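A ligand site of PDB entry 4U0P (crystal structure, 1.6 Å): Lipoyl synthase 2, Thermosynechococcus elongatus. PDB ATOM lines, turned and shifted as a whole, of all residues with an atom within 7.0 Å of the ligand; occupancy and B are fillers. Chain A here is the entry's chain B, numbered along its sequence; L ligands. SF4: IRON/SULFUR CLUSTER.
The side-chain hydroxyl (OG) of Ser 283 binds an iron atom (FE4) of the ligand, 2.0 Å away.
An iron atom (FE3) of the ligand is bound by the side-chain sulfur (SG) of Cys 42 (2.3 Å).
The side-chain sulfur of Cys 37 is bound to an iron atom (FE2) of the ligand, 2.3 Å away.
The side-chain sulfur (SG) of Cys 48 is bound to an iron atom (FE1) of the ligand, at 2.3 Å.
A sulfur (S3) of the ligand lies close to the side-chain hydroxyl (OG1) of Thr 55 (3.4 Å).
ND2 of Asn 44 lies close to S2 of the ligand (3.6 Å).
S4 of the ligand lies close to N of Arg 45, 3.7 Å away.
The side-chain hydroxyl (OG) of Ser 283 lies close to the side-chain hydroxyl (OG1) of Thr 55 (3.2 Å).
The backbone NH of Asn 44 sits close to the side-chain sulfur of Cys 42.
NH2 of Arg 281 sits close to SG of Cys 42.
N of Thr 55 lies close to SG of Cys 37.
The side-chain sulfur of Cys 48 sits close to the backbone carbonyl oxygen of Asn 44 (3.7 Å).
O of Thr 55 is in hydrogen-bond range of N of Ile 36, at 2.9 Å.
The side-chain amide nitrogen (ND2) of Asn 44 sits at hydrogen-bond distance from the backbone carbonyl oxygen (O) of Leu 279, at 2.9 Å.
The guanidinium group (NH1) of Arg 45 is in salt-bridge range of the side-chain carboxylate (OE2) of Glu 38.
Ile 36 touches the ligand (CG2 to S1, 3.9 Å).
Arg 281 touches the ligand (CB to S2, 3.9 Å).
Tyr 284 touches the ligand (CA to S2, 3.9 Å).
Within 4 Å of the ligand: Ile 36, Cys 37, Cys 42, Asn 44, Arg 45, Cys 48, Thr 55, Arg 281, Ser 283 and Tyr 284.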
ATOM      1  N   THR A  35     -18.707   6.119 -28.506  1.00  0.00           N
ATOM      2  CA  THR A  35     -18.570   5.951 -27.061  1.00  0.00           C
ATOM      3  C   THR A  35     -17.428   6.772 -26.510  1.00  0.00           C
ATOM      4  O   THR A  35     -16.439   7.041 -27.190  1.00  0.00           O
ATOM      5  CB  THR A  35     -18.280   4.524 -26.690  1.00  0.00           C
ATOM      6  OG1 THR A  35     -17.072   4.121 -27.342  1.00  0.00           O
ATOM      7  CG2 THR A  35     -19.427   3.606 -27.095  1.00  0.00           C
ATOM      8  N   ILE A  36     -17.591   7.208 -25.272  1.00  0.00           N
ATOM      9  CA  ILE A  36     -16.500   7.870 -24.557  1.00  0.00           C
ATOM     10  C   ILE A  36     -15.306   6.921 -24.491  1.00  0.00           C
ATOM     11  O   ILE A  36     -14.125   7.371 -24.562  1.00  0.00           O
ATOM     12  CB  ILE A  36     -16.977   8.259 -23.148  1.00  0.00           C
ATOM     13  CG1 ILE A  36     -18.058   9.343 -23.295  1.00  0.00           C
ATOM     14  CG2 ILE A  36     -15.803   8.703 -22.278  1.00  0.00           C
ATOM     15  CD1 ILE A  36     -17.589  10.658 -23.881  1.00  0.00           C
ATOM     16  N   CYS A  37     -15.576   5.639 -24.306  1.00  0.00           N
ATOM     17  CA  CYS A  37     -14.547   4.617 -24.166  1.00  0.00           C
ATOM     18  C   CYS A  37     -13.582   4.705 -25.340  1.00  0.00           C
ATOM     19  O   CYS A  37     -12.352   4.696 -25.151  1.00  0.00           O
ATOM     20  CB  CYS A  37     -15.171   3.226 -24.090  1.00  0.00           C
ATOM     21  SG  CYS A  37     -16.669   3.080 -23.031  1.00  0.00           S
ATOM     22  N   GLU A  38     -14.130   4.771 -26.546  1.00  0.00           N
ATOM     23  CA  GLU A  38     -13.329   4.838 -27.756  1.00  0.00           C
ATOM     24  C   GLU A  38     -12.851   6.259 -28.095  1.00  0.00           C
ATOM     25  O   GLU A  38     -11.705   6.429 -28.505  1.00  0.00           O
ATOM     26  CB  GLU A  38     -14.119   4.217 -28.926  1.00  0.00           C
ATOM     27  CG  GLU A  38     -14.278   2.682 -28.776  1.00  0.00           C
ATOM     28  CD  GLU A  38     -12.933   1.941 -28.733  1.00  0.00           C
ATOM     29  OE1 GLU A  38     -12.042   2.276 -29.556  1.00  0.00           O
ATOM     30  OE2 GLU A  38     -12.757   1.031 -27.867  1.00  0.00           O
ATOM     31  N   ARG A  41      -9.863   6.655 -25.822  1.00  0.00           N
ATOM     32  CA  ARG A  41      -8.964   5.517 -25.650  1.00  0.00           C
ATOM     33  C   ARG A  41      -8.801   5.175 -24.170  1.00  0.00           C
ATOM     34  O   ARG A  41      -7.695   5.111 -23.663  1.00  0.00           O
ATOM     35  CB  ARG A  41      -7.581   5.827 -26.248  1.00  0.00           C
ATOM     36  CG  ARG A  41      -7.553   5.913 -27.748  1.00  0.00           C
ATOM     37  CD  ARG A  41      -6.133   5.833 -28.243  1.00  0.00           C
ATOM     38  NE  ARG A  41      -6.015   6.182 -29.657  1.00  0.00           N
ATOM     39  CZ  ARG A  41      -4.854   6.449 -30.259  1.00  0.00           C
ATOM     40  NH1 ARG A  41      -3.716   6.401 -29.565  1.00  0.00           N
ATOM     41  NH2 ARG A  41      -4.842   6.753 -31.553  1.00  0.00           N
ATOM     42  N   CYS A  42      -9.917   4.998 -23.484  1.00  0.00           N
ATOM     43  CA  CYS A  42      -9.921   4.786 -22.050  1.00  0.00           C
ATOM     44  C   CYS A  42      -9.125   3.577 -21.621  1.00  0.00           C
ATOM     45  O   CYS A  42      -9.235   2.492 -22.208  1.00  0.00           O
ATOM     46  CB  CYS A  42     -11.354   4.648 -21.526  1.00  0.00           C
ATOM     47  SG  CYS A  42     -11.441   4.584 -19.722  1.00  0.00           S
ATOM     48  N   PRO A  43      -8.290   3.753 -20.585  1.00  0.00           N
ATOM     49  CA  PRO A  43      -7.449   2.644 -20.167  1.00  0.00           C
ATOM     50  C   PRO A  43      -8.210   1.545 -19.449  1.00  0.00           C
ATOM     51  O   PRO A  43      -7.649   0.490 -19.177  1.00  0.00           O
ATOM     52  CB  PRO A  43      -6.474   3.329 -19.203  1.00  0.00           C
ATOM     53  CG  PRO A  43      -7.201   4.461 -18.687  1.00  0.00           C
ATOM     54  CD  PRO A  43      -8.003   4.980 -19.817  1.00  0.00           C
ATOM     55  N   ASN A  44      -9.485   1.784 -19.155  1.00  0.00           N
ATOM     56  CA  ASN A  44     -10.298   0.768 -18.510  1.00  0.00           C
ATOM     57  C   ASN A  44     -11.075  -0.148 -19.452  1.00  0.00           C
ATOM     58  O   ASN A  44     -11.813  -0.996 -19.003  1.00  0.00           O
ATOM     59  CB  ASN A  44     -11.262   1.396 -17.510  1.00  0.00           C
ATOM     60  CG  ASN A  44     -10.551   2.168 -16.417  1.00  0.00           C
ATOM     61  OD1 ASN A  44      -9.561   1.653 -15.859  1.00  0.00           O
ATOM     62  ND2 ASN A  44     -11.013   3.363 -16.114  1.00  0.00           N
ATOM     63  N   ARG A  45     -10.922   0.037 -20.746  1.00  0.00           N
ATOM     64  CA  ARG A  45     -11.718  -0.712 -21.711  1.00  0.00           C
ATOM     65  C   ARG A  45     -11.681  -2.212 -21.539  1.00  0.00           C
ATOM     66  O   ARG A  45     -12.715  -2.886 -21.631  1.00  0.00           O
ATOM     67  CB  ARG A  45     -11.345  -0.330 -23.134  1.00  0.00           C
ATOM     68  CG  ARG A  45     -11.897   0.977 -23.557  1.00  0.00           C
ATOM     69  CD  ARG A  45     -11.393   1.404 -24.925  1.00  0.00           C
ATOM     70  NE  ARG A  45      -9.952   1.689 -24.894  1.00  0.00           N
ATOM     71  CZ  ARG A  45      -9.172   1.814 -25.972  1.00  0.00           C
ATOM     72  NH1 ARG A  45      -9.683   1.681 -27.187  1.00  0.00           N
ATOM     73  NH2 ARG A  45      -7.885   2.081 -25.821  1.00  0.00           N
ATOM     74  N   GLY A  46     -10.504  -2.778 -21.270  1.00  0.00           N
ATOM     75  CA  GLY A  46     -10.442  -4.216 -21.139  1.00  0.00           C
ATOM     76  C   GLY A  46     -11.393  -4.690 -20.059  1.00  0.00           C
ATOM     77  O   GLY A  46     -12.148  -5.655 -20.279  1.00  0.00           O
ATOM     78  N   GLU A  47     -11.348  -4.021 -18.912  1.00  0.00           N
ATOM     79  CA  GLU A  47     -12.150  -4.412 -17.759  1.00  0.00           C
ATOM     80  C   GLU A  47     -13.650  -4.110 -18.002  1.00  0.00           C
ATOM     81  O   GLU A  47     -14.504  -4.972 -17.784  1.00  0.00           O
ATOM     82  CB  GLU A  47     -11.705  -3.713 -16.496  1.00  0.00           C
ATOM     83  CG  GLU A  47     -12.453  -4.198 -15.264  1.00  0.00           C
ATOM     84  CD  GLU A  47     -11.799  -3.709 -13.975  1.00  0.00           C
ATOM     85  OE1 GLU A  47     -10.828  -2.913 -14.039  1.00  0.00           O
ATOM     86  OE2 GLU A  47     -12.277  -4.134 -12.891  1.00  0.00           O
ATOM     87  N   CYS A  48     -13.961  -2.906 -18.450  1.00  0.00           N
ATOM     88  CA  CYS A  48     -15.376  -2.567 -18.665  1.00  0.00           C
ATOM     89  C   CYS A  48     -16.022  -3.413 -19.775  1.00  0.00           C
ATOM     90  O   CYS A  48     -17.141  -3.916 -19.598  1.00  0.00           O
ATOM     91  CB  CYS A  48     -15.534  -1.062 -18.924  1.00  0.00           C
ATOM     92  SG  CYS A  48     -15.056  -0.024 -17.516  1.00  0.00           S
ATOM     93  N   TYR A  49     -15.363  -3.540 -20.913  1.00  0.00           N
ATOM     94  CA  TYR A  49     -15.933  -4.276 -22.024  1.00  0.00           C
ATOM     95  C   TYR A  49     -16.124  -5.696 -21.520  1.00  0.00           C
ATOM     96  O   TYR A  49     -17.101  -6.388 -21.866  1.00  0.00           O
ATOM     97  CB  TYR A  49     -15.004  -4.263 -23.219  1.00  0.00           C
ATOM     98  CG  TYR A  49     -14.873  -2.963 -23.969  1.00  0.00           C
ATOM     99  CD1 TYR A  49     -15.561  -1.827 -23.567  1.00  0.00           C
ATOM    100  CD2 TYR A  49     -14.082  -2.863 -25.091  1.00  0.00           C
ATOM    101  CE1 TYR A  49     -15.443  -0.642 -24.283  1.00  0.00           C
ATOM    102  CE2 TYR A  49     -13.961  -1.714 -25.800  1.00  0.00           C
ATOM    103  CZ  TYR A  49     -14.654  -0.582 -25.390  1.00  0.00           C
ATOM    104  OH  TYR A  49     -14.545   0.583 -26.097  1.00  0.00           O
ATOM    105  N   THR A  53     -20.190  -3.423 -20.130  1.00  0.00           N
ATOM    106  CA  THR A  53     -20.634  -2.036 -19.942  1.00  0.00           C
ATOM    107  C   THR A  53     -19.931  -1.141 -20.946  1.00  0.00           C
ATOM    108  O   THR A  53     -18.862  -1.466 -21.432  1.00  0.00           O
ATOM    109  CB  THR A  53     -20.339  -1.543 -18.554  1.00  0.00           C
ATOM    110  OG1 THR A  53     -20.819  -2.477 -17.588  1.00  0.00           O
ATOM    111  CG2 THR A  53     -21.004  -0.220 -18.305  1.00  0.00           C
ATOM    112  N   ALA A  54     -20.531  -0.007 -21.285  1.00  0.00           N
ATOM    113  CA  ALA A  54     -19.875   0.983 -22.103  1.00  0.00           C
ATOM    114  C   ALA A  54     -20.585   2.309 -21.839  1.00  0.00           C
ATOM    115  O   ALA A  54     -21.646   2.309 -21.232  1.00  0.00           O
ATOM    116  CB  ALA A  54     -19.955   0.656 -23.489  1.00  0.00           C
ATOM    117  N   THR A  55     -19.974   3.412 -22.272  1.00  0.00           N
ATOM    118  CA  THR A  55     -20.538   4.772 -22.113  1.00  0.00           C
ATOM    119  C   THR A  55     -20.700   5.398 -23.507  1.00  0.00           C
ATOM    120  O   THR A  55     -19.732   5.628 -24.218  1.00  0.00           O
ATOM    121  CB  THR A  55     -19.609   5.624 -21.260  1.00  0.00           C
ATOM    122  OG1 THR A  55     -19.552   5.103 -19.930  1.00  0.00           O
ATOM    123  CG2 THR A  55     -20.175   7.037 -21.123  1.00  0.00           C
ATOM    124  N   GLN A  71     -11.781  15.604 -22.870  1.00  0.00           N
ATOM    125  CA  GLN A  71     -11.231  14.831 -23.967  1.00  0.00           C
ATOM    126  C   GLN A  71     -12.066  14.782 -25.235  1.00  0.00           C
ATOM    127  O   GLN A  71     -11.604  14.300 -26.252  1.00  0.00           O
ATOM    128  CB  GLN A  71     -10.983  13.374 -23.509  1.00  0.00           C
ATOM    129  CG  GLN A  71     -12.235  12.602 -23.095  1.00  0.00           C
ATOM    130  CD  GLN A  71     -11.893  11.310 -22.327  1.00  0.00           C
ATOM    131  OE1 GLN A  71     -10.746  10.827 -22.342  1.00  0.00           O
ATOM    132  NE2 GLN A  71     -12.887  10.767 -21.618  1.00  0.00           N
ATOM    133  N   VAL A 102     -24.096   3.389 -19.778  1.00  0.00           N
ATOM    134  CA  VAL A 102     -24.093   4.790 -19.344  1.00  0.00           C
ATOM    135  C   VAL A 102     -24.336   5.651 -20.571  1.00  0.00           C
ATOM    136  O   VAL A 102     -23.777   5.401 -21.638  1.00  0.00           O
ATOM    137  CB  VAL A 102     -22.763   5.148 -18.686  1.00  0.00           C
ATOM    138  CG1 VAL A 102     -22.793   6.604 -18.291  1.00  0.00           C
ATOM    139  CG2 VAL A 102     -22.549   4.269 -17.496  1.00  0.00           C
ATOM    140  N   LEU A 279      -7.095   5.543 -11.890  1.00  0.00           N
ATOM    141  CA  LEU A 279      -7.722   5.353 -13.184  1.00  0.00           C
ATOM    142  C   LEU A 279      -9.222   5.300 -13.088  1.00  0.00           C
ATOM    143  O   LEU A 279      -9.878   5.044 -14.095  1.00  0.00           O
ATOM    144  CB  LEU A 279      -7.176   4.103 -13.895  1.00  0.00           C
ATOM    145  CG  LEU A 279      -5.706   4.257 -14.304  1.00  0.00           C
ATOM    146  CD1 LEU A 279      -5.335   3.190 -15.262  1.00  0.00           C
ATOM    147  CD2 LEU A 279      -5.377   5.621 -14.939  1.00  0.00           C
ATOM    148  N   VAL A 280      -9.798   5.562 -11.911  1.00  0.00           N
ATOM    149  CA  VAL A 280     -11.268   5.670 -11.802  1.00  0.00           C
ATOM    150  C   VAL A 280     -11.827   6.770 -12.686  1.00  0.00           C
ATOM    151  O   VAL A 280     -11.251   7.848 -12.789  1.00  0.00           O
ATOM    152  CB  VAL A 280     -11.691   5.879 -10.334  1.00  0.00           C
ATOM    153  CG1 VAL A 280     -13.176   6.227 -10.207  1.00  0.00           C
ATOM    154  CG2 VAL A 280     -11.389   4.639  -9.510  1.00  0.00           C
ATOM    155  N   ARG A 281     -12.953   6.479 -13.338  1.00  0.00           N
ATOM    156  CA  ARG A 281     -13.694   7.456 -14.158  1.00  0.00           C
ATOM    157  C   ARG A 281     -15.151   7.376 -13.753  1.00  0.00           C
ATOM    158  O   ARG A 281     -15.525   6.440 -13.057  1.00  0.00           O
ATOM    159  CB  ARG A 281     -13.556   7.130 -15.639  1.00  0.00           C
ATOM    160  CG  ARG A 281     -12.147   7.058 -16.161  1.00  0.00           C
ATOM    161  CD  ARG A 281     -11.520   8.417 -16.266  1.00  0.00           C
ATOM    162  NE  ARG A 281     -10.062   8.341 -16.402  1.00  0.00           N
ATOM    163  CZ  ARG A 281      -9.418   8.103 -17.556  1.00  0.00           C
ATOM    164  NH1 ARG A 281      -8.083   8.080 -17.542  1.00  0.00           N
ATOM    165  NH2 ARG A 281     -10.099   7.880 -18.696  1.00  0.00           N
ATOM    166  N   SER A 282     -15.974   8.359 -14.165  1.00  0.00           N
ATOM    167  CA  SER A 282     -17.392   8.400 -13.777  1.00  0.00           C
ATOM    168  C   SER A 282     -18.166   7.087 -13.964  1.00  0.00           C
ATOM    169  O   SER A 282     -19.017   6.746 -13.148  1.00  0.00           O
ATOM    170  CB  SER A 282     -18.107   9.509 -14.576  1.00  0.00           C
ATOM    171  OG  SER A 282     -17.573  10.770 -14.332  1.00  0.00           O
ATOM    172  N   SER A 283     -17.862   6.363 -15.041  1.00  0.00           N
ATOM    173  CA  SER A 283     -18.582   5.164 -15.426  1.00  0.00           C
ATOM    174  C   SER A 283     -17.924   3.871 -14.964  1.00  0.00           C
ATOM    175  O   SER A 283     -18.429   2.775 -15.232  1.00  0.00           O
ATOM    176  CB  SER A 283     -18.677   5.121 -16.959  1.00  0.00           C
ATOM    177  OG  SER A 283     -17.455   5.619 -17.520  1.00  0.00           O
ATOM    178  N   TYR A 284     -16.777   4.012 -14.305  1.00  0.00           N
ATOM    179  CA  TYR A 284     -15.977   2.852 -13.936  1.00  0.00           C
ATOM    180  C   TYR A 284     -16.667   2.094 -12.815  1.00  0.00           C
ATOM    181  O   TYR A 284     -16.892   2.650 -11.734  1.00  0.00           O
ATOM    182  CB  TYR A 284     -14.576   3.288 -13.485  1.00  0.00           C
ATOM    183  CG  TYR A 284     -13.650   2.129 -13.173  1.00  0.00           C
ATOM    184  CD1 TYR A 284     -13.299   1.241 -14.161  1.00  0.00           C
ATOM    185  CD2 TYR A 284     -13.142   1.949 -11.886  1.00  0.00           C
ATOM    186  CE1 TYR A 284     -12.449   0.155 -13.888  1.00  0.00           C
ATOM    187  CE2 TYR A 284     -12.307   0.887 -11.596  1.00  0.00           C
ATOM    188  CZ  TYR A 284     -11.976  -0.002 -12.595  1.00  0.00           C
ATOM    189  OH  TYR A 284     -11.135  -1.072 -12.306  1.00  0.00           O
ATOM    190  N   HIS A 285     -16.968   0.836 -13.071  1.00  0.00           N
ATOM    191  CA  HIS A 285     -17.666  -0.048 -12.132  1.00  0.00           C
ATOM    192  C   HIS A 285     -19.026   0.519 -11.738  1.00  0.00           C
ATOM    193  O   HIS A 285     -19.516   0.323 -10.629  1.00  0.00           O
ATOM    194  CB  HIS A 285     -16.809  -0.309 -10.889  1.00  0.00           C
ATOM    195  CG  HIS A 285     -15.698  -1.288 -11.145  1.00  0.00           C
ATOM    196  ND1 HIS A 285     -14.775  -1.632 -10.184  1.00  0.00           N
ATOM    197  CD2 HIS A 285     -15.368  -1.974 -12.263  1.00  0.00           C
ATOM    198  CE1 HIS A 285     -13.937  -2.513 -10.696  1.00  0.00           C
ATOM    199  NE2 HIS A 285     -14.263  -2.728 -11.956  1.00  0.00           N
HETATM  200 FE1  SF4 L   1     -15.227   2.004 -18.582  1.00  0.00          FE
HETATM  201 FE2  SF4 L   1     -15.778   3.323 -20.944  1.00  0.00          FE
HETATM  202 FE3  SF4 L   1     -13.616   4.009 -19.497  1.00  0.00          FE
HETATM  203 FE4  SF4 L   1     -16.095   4.517 -18.469  1.00  0.00          FE
HETATM  204  S1  SF4 L   1     -15.195   5.373 -20.274  1.00  0.00           S
HETATM  205  S2  SF4 L   1     -14.324   3.738 -17.408  1.00  0.00           S
HETATM  206  S3  SF4 L   1     -17.198   2.744 -19.321  1.00  0.00           S
HETATM  207  S4  SF4 L   1     -14.034   2.019 -20.483  1.00  0.00           S
